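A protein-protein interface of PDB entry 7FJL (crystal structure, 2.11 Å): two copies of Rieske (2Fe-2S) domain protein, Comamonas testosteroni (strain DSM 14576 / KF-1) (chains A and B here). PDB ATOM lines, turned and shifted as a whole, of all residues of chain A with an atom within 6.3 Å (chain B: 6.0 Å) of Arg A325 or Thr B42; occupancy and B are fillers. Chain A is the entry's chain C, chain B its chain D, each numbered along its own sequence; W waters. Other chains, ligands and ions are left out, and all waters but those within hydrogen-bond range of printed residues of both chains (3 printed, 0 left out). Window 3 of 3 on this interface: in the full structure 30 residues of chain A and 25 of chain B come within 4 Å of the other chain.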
ATOM      1  N   GLN A 323      29.583 -20.015 -34.020  1.00  0.00           N
ATOM      2  CA  GLN A 323      28.686 -19.113 -33.312  1.00  0.00           C
ATOM      3  C   GLN A 323      28.314 -17.940 -34.225  1.00  0.00           C
ATOM      4  O   GLN A 323      29.180 -17.324 -34.841  1.00  0.00           O
ATOM      5  CB  GLN A 323      29.334 -18.580 -32.036  1.00  0.00           C
ATOM      6  CG  GLN A 323      28.471 -17.519 -31.297  1.00  0.00           C
ATOM      7  CD  GLN A 323      29.057 -17.163 -29.943  1.00  0.00           C
ATOM      8  OE1 GLN A 323      30.126 -16.554 -29.825  1.00  0.00           O
ATOM      9  NE2 GLN A 323      28.409 -17.576 -28.888  1.00  0.00           N
ATOM     10  N   ASP A 324      27.045 -17.541 -34.174  1.00  0.00           N
ATOM     11  CA  ASP A 324      26.524 -16.523 -35.066  1.00  0.00           C
ATOM     12  C   ASP A 324      26.192 -15.271 -34.249  1.00  0.00           C
ATOM     13  O   ASP A 324      25.176 -15.239 -33.560  1.00  0.00           O
ATOM     14  CB  ASP A 324      25.350 -17.113 -35.866  1.00  0.00           C
ATOM     15  CG  ASP A 324      24.851 -16.161 -36.944  1.00  0.00           C
ATOM     16  OD1 ASP A 324      24.579 -16.642 -38.029  1.00  0.00           O
ATOM     17  OD2 ASP A 324      24.746 -14.961 -36.699  1.00  0.00           O
ATOM     18  N   ARG A 325      27.023 -14.225 -34.328  1.00  0.00           N
ATOM     19  CA  ARG A 325      26.793 -13.062 -33.464  1.00  0.00           C
ATOM     20  C   ARG A 325      25.489 -12.347 -33.849  1.00  0.00           C
ATOM     21  O   ARG A 325      24.803 -11.757 -32.994  1.00  0.00           O
ATOM     22  CB  ARG A 325      28.021 -12.146 -33.516  1.00  0.00           C
ATOM     23  CG  ARG A 325      29.238 -12.729 -32.803  1.00  0.00           C
ATOM     24  CD  ARG A 325      28.722 -12.390 -31.420  1.00  0.00           C
ATOM     25  NE  ARG A 325      29.317 -13.192 -30.411  1.00  0.00           N
ATOM     26  CZ  ARG A 325      29.110 -13.098 -29.090  1.00  0.00           C
ATOM     27  NH1 ARG A 325      28.331 -12.179 -28.528  1.00  0.00           N
ATOM     28  NH2 ARG A 325      29.766 -13.957 -28.369  1.00  0.00           N
ATOM     29  N   ASN A 326      25.139 -12.388 -35.152  1.00  0.00           N
ATOM     30  CA  ASN A 326      23.889 -11.751 -35.594  1.00  0.00           C
ATOM     31  C   ASN A 326      22.673 -12.527 -35.070  1.00  0.00           C
ATOM     32  O   ASN A 326      21.687 -11.926 -34.637  1.00  0.00           O
ATOM     33  CB  ASN A 326      23.831 -11.539 -37.121  1.00  0.00           C
ATOM     34  CG  ASN A 326      24.817 -10.497 -37.611  1.00  0.00           C
ATOM     35  OD1 ASN A 326      24.971  -9.456 -37.008  1.00  0.00           O
ATOM     36  ND2 ASN A 326      25.474 -10.732 -38.727  1.00  0.00           N
ATOM     37  N   ALA A 327      22.732 -13.863 -35.083  1.00  0.00           N
ATOM     38  CA  ALA A 327      21.675 -14.609 -34.409  1.00  0.00           C
ATOM     39  C   ALA A 327      21.527 -14.130 -32.951  1.00  0.00           C
ATOM     40  O   ALA A 327      20.431 -13.927 -32.431  1.00  0.00           O
ATOM     41  CB  ALA A 327      21.951 -16.099 -34.512  1.00  0.00           C
ATOM     42  N   MET A 328      22.663 -13.867 -32.289  1.00  0.00           N
ATOM     43  CA  MET A 328      22.616 -13.569 -30.877  1.00  0.00           C
ATOM     44  C   MET A 328      22.001 -12.194 -30.662  1.00  0.00           C
ATOM     45  O   MET A 328      21.171 -12.028 -29.744  1.00  0.00           O
ATOM     46  CB  MET A 328      23.994 -13.667 -30.209  1.00  0.00           C
ATOM     47  CG  MET A 328      24.567 -15.075 -30.161  1.00  0.00           C
ATOM     48  SD  MET A 328      26.308 -14.947 -29.623  1.00  0.00           S
ATOM     49  CE  MET A 328      26.034 -14.732 -27.862  1.00  0.00           C
ATOM     50  N   LYS A 329      22.372 -11.265 -31.549  1.00  0.00           N
ATOM     51  CA  LYS A 329      21.773  -9.941 -31.543  1.00  0.00           C
ATOM     52  C   LYS A 329      20.277 -10.041 -31.817  1.00  0.00           C
ATOM     53  O   LYS A 329      19.494  -9.345 -31.187  1.00  0.00           O
ATOM     54  CB  LYS A 329      22.453  -9.036 -32.565  1.00  0.00           C
ATOM     55  CG  LYS A 329      22.668  -7.618 -32.082  1.00  0.00           C
ATOM     56  CD  LYS A 329      21.584  -6.688 -32.541  1.00  0.00           C
ATOM     57  CE  LYS A 329      22.173  -5.361 -32.979  1.00  0.00           C
ATOM     58  NZ  LYS A 329      23.157  -4.899 -31.969  1.00  0.00           N
ATOM     59  N   ALA A 330      19.872 -10.999 -32.662  1.00  0.00           N
ATOM     60  CA  ALA A 330      18.465 -11.170 -32.956  1.00  0.00           C
ATOM     61  C   ALA A 330      17.720 -11.767 -31.758  1.00  0.00           C
ATOM     62  O   ALA A 330      16.511 -11.802 -31.790  1.00  0.00           O
ATOM     63  CB  ALA A 330      18.258 -11.984 -34.217  1.00  0.00           C
ATOM     64  N   THR A 334      22.779 -18.297 -27.592  1.00  0.00           N
ATOM     65  CA  THR A 334      24.169 -18.668 -27.816  1.00  0.00           C
ATOM     66  C   THR A 334      24.634 -18.469 -29.258  1.00  0.00           C
ATOM     67  O   THR A 334      25.823 -18.299 -29.492  1.00  0.00           O
ATOM     68  CB  THR A 334      24.364 -20.161 -27.533  1.00  0.00           C
ATOM     69  OG1 THR A 334      23.773 -20.911 -28.602  1.00  0.00           O
ATOM     70  CG2 THR A 334      23.755 -20.596 -26.203  1.00  0.00           C
ATOM     71  N   GLY A 335      23.745 -18.499 -30.251  1.00  0.00           N
ATOM     72  CA  GLY A 335      24.172 -18.334 -31.637  1.00  0.00           C
ATOM     73  C   GLY A 335      24.802 -19.607 -32.181  1.00  0.00           C
ATOM     74  O   GLY A 335      25.401 -19.622 -33.272  1.00  0.00           O
ATOM     75  N   GLU B  35      39.123  -3.748 -33.301  1.00  0.00           N
ATOM     76  CA  GLU B  35      38.660  -5.105 -33.085  1.00  0.00           C
ATOM     77  C   GLU B  35      37.393  -5.112 -32.198  1.00  0.00           C
ATOM     78  O   GLU B  35      36.595  -6.030 -32.289  1.00  0.00           O
ATOM     79  CB  GLU B  35      39.741  -5.980 -32.432  1.00  0.00           C
ATOM     80  CG  GLU B  35      40.855  -6.406 -33.374  1.00  0.00           C
ATOM     81  CD  GLU B  35      42.012  -7.011 -32.583  1.00  0.00           C
ATOM     82  OE1 GLU B  35      41.882  -8.176 -32.172  1.00  0.00           O
ATOM     83  OE2 GLU B  35      43.083  -6.323 -32.377  1.00  0.00           O
ATOM     84  N   VAL B  36      37.214  -4.122 -31.323  1.00  0.00           N
ATOM     85  CA  VAL B  36      36.226  -4.285 -30.274  1.00  0.00           C
ATOM     86  C   VAL B  36      34.860  -3.765 -30.724  1.00  0.00           C
ATOM     87  O   VAL B  36      33.853  -4.081 -30.083  1.00  0.00           O
ATOM     88  CB  VAL B  36      36.671  -3.705 -28.916  1.00  0.00           C
ATOM     89  CG1 VAL B  36      37.998  -4.317 -28.539  1.00  0.00           C
ATOM     90  CG2 VAL B  36      36.726  -2.179 -28.922  1.00  0.00           C
ATOM     91  N   GLY B  37      34.841  -3.001 -31.830  1.00  0.00           N
ATOM     92  CA  GLY B  37      33.570  -2.628 -32.432  1.00  0.00           C
ATOM     93  C   GLY B  37      32.812  -1.565 -31.624  1.00  0.00           C
ATOM     94  O   GLY B  37      33.411  -0.756 -30.927  1.00  0.00           O
ATOM     95  N   GLU B  38      31.494  -1.554 -31.764  1.00  0.00           N
ATOM     96  CA  GLU B  38      30.656  -0.559 -31.093  1.00  0.00           C
ATOM     97  C   GLU B  38      30.262  -1.059 -29.699  1.00  0.00           C
ATOM     98  O   GLU B  38      30.601  -2.181 -29.344  1.00  0.00           O
ATOM     99  CB  GLU B  38      29.384  -0.305 -31.915  1.00  0.00           C
ATOM    100  CG  GLU B  38      29.708   0.096 -33.344  1.00  0.00           C
ATOM    101  CD  GLU B  38      30.532   1.374 -33.291  1.00  0.00           C
ATOM    102  OE1 GLU B  38      31.630   1.404 -33.909  1.00  0.00           O
ATOM    103  OE2 GLU B  38      30.110   2.333 -32.585  1.00  0.00           O
ATOM    104  N   ASP B  40      28.418  -3.002 -26.971  1.00  0.00           N
ATOM    105  CA  ASP B  40      27.770  -4.305 -27.035  1.00  0.00           C
ATOM    106  C   ASP B  40      28.314  -5.086 -28.220  1.00  0.00           C
ATOM    107  O   ASP B  40      27.614  -5.963 -28.714  1.00  0.00           O
ATOM    108  CB  ASP B  40      26.264  -4.189 -27.221  1.00  0.00           C
ATOM    109  CG  ASP B  40      25.590  -3.584 -26.001  1.00  0.00           C
ATOM    110  OD1 ASP B  40      24.415  -3.166 -26.098  1.00  0.00           O
ATOM    111  OD2 ASP B  40      26.215  -3.585 -24.953  1.00  0.00           O
ATOM    112  N   GLY B  41      29.503  -4.705 -28.719  1.00  0.00           N
ATOM    113  CA  GLY B  41      30.174  -5.398 -29.806  1.00  0.00           C
ATOM    114  C   GLY B  41      30.583  -6.843 -29.459  1.00  0.00           C
ATOM    115  O   GLY B  41      30.597  -7.261 -28.272  1.00  0.00           O
ATOM    116  N   THR B  42      30.925  -7.604 -30.517  1.00  0.00           N
ATOM    117  CA  THR B  42      31.373  -8.988 -30.412  1.00  0.00           C
ATOM    118  C   THR B  42      32.578  -9.031 -29.460  1.00  0.00           C
ATOM    119  O   THR B  42      33.470  -8.217 -29.627  1.00  0.00           O
ATOM    120  CB  THR B  42      31.771  -9.501 -31.786  1.00  0.00           C
ATOM    121  OG1 THR B  42      30.555  -9.440 -32.558  1.00  0.00           O
ATOM    122  CG2 THR B  42      32.256 -10.931 -31.734  1.00  0.00           C
ATOM    123  N   PRO B  43      32.611  -9.899 -28.409  1.00  0.00           N
ATOM    124  CA  PRO B  43      33.817 -10.083 -27.584  1.00  0.00           C
ATOM    125  C   PRO B  43      35.026 -10.521 -28.410  1.00  0.00           C
ATOM    126  O   PRO B  43      34.889 -11.303 -29.367  1.00  0.00           O
ATOM    127  CB  PRO B  43      33.454 -11.100 -26.487  1.00  0.00           C
ATOM    128  CG  PRO B  43      31.921 -11.073 -26.510  1.00  0.00           C
ATOM    129  CD  PRO B  43      31.481 -10.713 -27.934  1.00  0.00           C
ATOM    130  N   VAL B  44      36.214 -10.061 -27.982  1.00  0.00           N
ATOM    131  CA  VAL B  44      37.477 -10.253 -28.715  1.00  0.00           C
ATOM    132  C   VAL B  44      38.373 -11.108 -27.808  1.00  0.00           C
ATOM    133  O   VAL B  44      38.377 -10.886 -26.604  1.00  0.00           O
ATOM    134  CB  VAL B  44      38.120  -8.864 -28.985  1.00  0.00           C
ATOM    135  CG1 VAL B  44      39.577  -8.973 -29.353  1.00  0.00           C
ATOM    136  CG2 VAL B  44      37.368  -8.092 -30.054  1.00  0.00           C
ATOM    137  N   VAL B  55      38.198  -9.133 -24.476  1.00  0.00           N
ATOM    138  CA  VAL B  55      38.110  -7.688 -24.517  1.00  0.00           C
ATOM    139  C   VAL B  55      36.733  -7.368 -25.063  1.00  0.00           C
ATOM    140  O   VAL B  55      36.290  -7.991 -26.033  1.00  0.00           O
ATOM    141  CB  VAL B  55      39.181  -7.069 -25.428  1.00  0.00           C
ATOM    142  CG1 VAL B  55      39.173  -5.523 -25.275  1.00  0.00           C
ATOM    143  CG2 VAL B  55      40.585  -7.626 -25.146  1.00  0.00           C
ATOM    144  N   PHE B  56      36.056  -6.401 -24.439  1.00  0.00           N
ATOM    145  CA  PHE B  56      34.726  -6.093 -24.910  1.00  0.00           C
ATOM    146  C   PHE B  56      34.376  -4.650 -24.569  1.00  0.00           C
ATOM    147  O   PHE B  56      34.869  -4.138 -23.549  1.00  0.00           O
ATOM    148  CB  PHE B  56      33.671  -7.040 -24.303  1.00  0.00           C
ATOM    149  CG  PHE B  56      33.334  -6.810 -22.851  1.00  0.00           C
ATOM    150  CD1 PHE B  56      34.191  -7.229 -21.841  1.00  0.00           C
ATOM    151  CD2 PHE B  56      32.142  -6.227 -22.469  1.00  0.00           C
ATOM    152  CE1 PHE B  56      33.859  -7.086 -20.501  1.00  0.00           C
ATOM    153  CE2 PHE B  56      31.843  -6.043 -21.125  1.00  0.00           C
ATOM    154  CZ  PHE B  56      32.672  -6.530 -20.141  1.00  0.00           C
ATOM    155  N   ARG B  57      33.458  -4.086 -25.378  1.00  0.00           N
ATOM    156  CA  ARG B  57      33.008  -2.722 -25.176  1.00  0.00           C
ATOM    157  C   ARG B  57      31.562  -2.821 -24.719  1.00  0.00           C
ATOM    158  O   ARG B  57      30.722  -3.366 -25.457  1.00  0.00           O
ATOM    159  CB  ARG B  57      33.163  -1.897 -26.456  1.00  0.00           C
ATOM    160  CG  ARG B  57      32.777  -0.425 -26.305  1.00  0.00           C
ATOM    161  CD  ARG B  57      32.727   0.491 -27.516  1.00  0.00           C
ATOM    162  NE  ARG B  57      33.990   0.576 -28.220  1.00  0.00           N
ATOM    163  CZ  ARG B  57      35.077   1.289 -27.842  1.00  0.00           C
ATOM    164  NH1 ARG B  57      35.092   2.020 -26.724  1.00  0.00           N
ATOM    165  NH2 ARG B  57      36.146   1.292 -28.630  1.00  0.00           N
ATOM    166  N   LEU B  77      34.590 -16.706 -21.916  1.00  0.00           N
ATOM    167  CA  LEU B  77      33.649 -15.601 -21.930  1.00  0.00           C
ATOM    168  C   LEU B  77      33.642 -14.952 -23.313  1.00  0.00           C
ATOM    169  O   LEU B  77      32.809 -14.074 -23.582  1.00  0.00           O
ATOM    170  CB  LEU B  77      34.072 -14.552 -20.897  1.00  0.00           C
ATOM    171  CG  LEU B  77      34.008 -14.975 -19.423  1.00  0.00           C
ATOM    172  CD1 LEU B  77      34.556 -13.855 -18.541  1.00  0.00           C
ATOM    173  CD2 LEU B  77      32.550 -15.311 -19.032  1.00  0.00           C
ATOM    174  N   VAL B  78      34.543 -15.417 -24.206  1.00  0.00           N
ATOM    175  CA  VAL B  78      34.593 -14.854 -25.556  1.00  0.00           C
ATOM    176  C   VAL B  78      33.243 -15.152 -26.214  1.00  0.00           C
ATOM    177  O   VAL B  78      32.723 -14.340 -27.023  1.00  0.00           O
ATOM    178  CB  VAL B  78      35.836 -15.372 -26.338  1.00  0.00           C
ATOM    179  CG1 VAL B  78      35.740 -15.161 -27.859  1.00  0.00           C
ATOM    180  CG2 VAL B  78      37.116 -14.745 -25.786  1.00  0.00           C
ATOM    181  N   TYR B  79      32.633 -16.282 -25.804  1.00  0.00           N
ATOM    182  CA  TYR B  79      31.348 -16.685 -26.385  1.00  0.00           C
ATOM    183  C   TYR B  79      30.141 -15.951 -25.784  1.00  0.00           C
ATOM    184  O   TYR B  79      29.020 -16.220 -26.211  1.00  0.00           O
ATOM    185  CB  TYR B  79      31.119 -18.202 -26.282  1.00  0.00           C
ATOM    186  CG  TYR B  79      32.149 -18.956 -27.077  1.00  0.00           C
ATOM    187  CD1 TYR B  79      31.863 -19.304 -28.401  1.00  0.00           C
ATOM    188  CD2 TYR B  79      33.431 -19.201 -26.553  1.00  0.00           C
ATOM    189  CE1 TYR B  79      32.837 -19.919 -29.177  1.00  0.00           C
ATOM    190  CE2 TYR B  79      34.414 -19.787 -27.334  1.00  0.00           C
ATOM    191  CZ  TYR B  79      34.112 -20.101 -28.658  1.00  0.00           C
ATOM    192  OH  TYR B  79      35.009 -20.714 -29.468  1.00  0.00           O
ATOM    193  N   GLY B  80      30.352 -15.054 -24.804  1.00  0.00           N
ATOM    194  CA  GLY B  80      29.243 -14.632 -23.950  1.00  0.00           C
ATOM    195  C   GLY B  80      28.433 -13.521 -24.601  1.00  0.00           C
ATOM    196  O   GLY B  80      28.773 -13.089 -25.707  1.00  0.00           O
ATOM    197  N   ARG B  81      27.380 -13.049 -23.892  1.00  0.00           N
ATOM    198  CA  ARG B  81      26.484 -12.024 -24.403  1.00  0.00           C
ATOM    199  C   ARG B  81      26.937 -10.687 -23.849  1.00  0.00           C
ATOM    200  O   ARG B  81      26.931 -10.487 -22.638  1.00  0.00           O
ATOM    201  CB  ARG B  81      25.040 -12.308 -24.002  1.00  0.00           C
ATOM    202  CG  ARG B  81      24.520 -13.618 -24.573  1.00  0.00           C
ATOM    203  CD  ARG B  81      23.014 -13.763 -24.394  1.00  0.00           C
ATOM    204  NE  ARG B  81      22.279 -12.664 -25.001  1.00  0.00           N
ATOM    205  CZ  ARG B  81      21.901 -12.626 -26.289  1.00  0.00           C
ATOM    206  NH1 ARG B  81      22.144 -13.668 -27.084  1.00  0.00           N
ATOM    207  NH2 ARG B  81      21.274 -11.545 -26.763  1.00  0.00           N
ATOM    208  N   ASN B  82      27.296  -9.775 -24.768  1.00  0.00           N
ATOM    209  CA  ASN B  82      27.775  -8.471 -24.380  1.00  0.00           C
ATOM    210  C   ASN B  82      26.593  -7.532 -24.563  1.00  0.00           C
ATOM    211  O   ASN B  82      26.303  -7.131 -25.680  1.00  0.00           O
ATOM    212  CB  ASN B  82      28.887  -8.080 -25.353  1.00  0.00           C
ATOM    213  CG  ASN B  82      29.442  -6.706 -25.036  1.00  0.00           C
ATOM    214  OD1 ASN B  82      29.087  -6.177 -23.997  1.00  0.00           O
ATOM    215  ND2 ASN B  82      30.334  -6.155 -25.856  1.00  0.00           N
HETATM  216  O   HOH W   1      27.841  -8.772 -29.158  1.00  0.00           O
HETATM  217  O   HOH W   2      19.971  -9.084 -28.544  1.00  0.00           O
HETATM  218  O   HOH W   3      24.875  -6.419 -29.501  1.00  0.00           O
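The backbone carbonyl oxygen (O) of Met A328 lies within hydrogen-bond range of the guanidinium group (NH2) of Arg B81, at 3.0 Å. The guanidinium group (NH2) of Arg A325 is in hydrogen-bond range of the backbone carbonyl oxygen (O) of Gly B80 (3.0 Å). NH2 of Arg A325 is in hydrogen-bond range of O of Val B78 (3.3 Å). NE2 of Gln A323 sits at hydrogen-bond distance from O of Tyr B79, at 3.1 Å. O of Tyr B79 sits at hydrogen-bond distance from NH2 of Arg A325 (3.2 Å).
The side-chain amide nitrogen of Gln A323 lies within hydrogen-bond range of the side-chain sulfur of Met A328, at 3.4 Å. The side-chain amide oxygen (OE1) of Gln A323 sits at hydrogen-bond distance from the guanidinium group (NH2) of Arg A325 (3.0 Å). The guanidinium group of Arg A325 sits close to the side-chain sulfur of Met A328. The side-chain amide nitrogen (NE2) of Gln A323 lies within hydrogen-bond range of the backbone carbonyl oxygen (O) of Thr A334 (2.8 Å).
Arg A325 touches Thr B42 (CG to OG1, 3.6 Å). Arg A325 touches Pro B43 (NH1 to CD, 3.5 Å). CE of Met A328 touches O of Tyr B79 (3.7 Å). Gly B80 touches Met A328.
Of chain B, only Thr B42 (3.6 Å), Pro B43 (3.5 Å), Val B78 (3.3 Å), Tyr B79 (3.2 Å) and Gly B80 (3.0 Å) come within 4 Å of Arg A325. Thr B42 touches just one residue of chain A: Arg A325. Of the printed residues of chain A, Pro B43 touches Arg A325 (3.5 Å). Printed residues of chain A within 4 Å of Val B78: Arg A325 (3.3 Å). Printed residues of chain A within 4 Å of Arg B81: Met A328 (3.0 Å). Asn B82 touches none of the printed residues of chain A. Phe B56 touches none of the printed residues of chain A. The nearest residue of chain B that does not touch Arg A325 is Arg B81 (4.5 Å). The nearest printed residue of chain A that does not touch Thr B42 is Gln A323 (6.3 Å). The nearest printed residue of chain A that does not touch Val B78 is Gln A323 (4.4 Å).
Hydrophobic or aromatic side chains of chain B that line the printed part of chain A: Pro B43 and Tyr B79. Of the 10 printed residues of chain A, 3 touch a printed residue of chain B. Hydrophobic or aromatic side chains of chain A that line the printed part of chain B: Met A328. Among the printed residues, no Asp or Glu carboxylate lies within 4 Å of a Lys or Arg side-chain nitrogen of the other chain.
No position is printed for both chains.
Water W2 lies within hydrogen-bond range of the backbone carbonyl oxygen of Lys A329 (2.7 Å), the guanidinium group of Arg B81 (3.3 Å) and the backbone carbonyl oxygen of Met A328 (3.4 Å). Water W1 lies within hydrogen-bond range of the backbone carbonyl oxygen of Asp B40 (2.9 Å), the backbone carbonyl oxygen of Gly B41 (3.3 Å) and the guanidinium group of Arg A325 (3.5 Å). Water W3 bridges O of Asp B40 and NZ of Lys A329.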
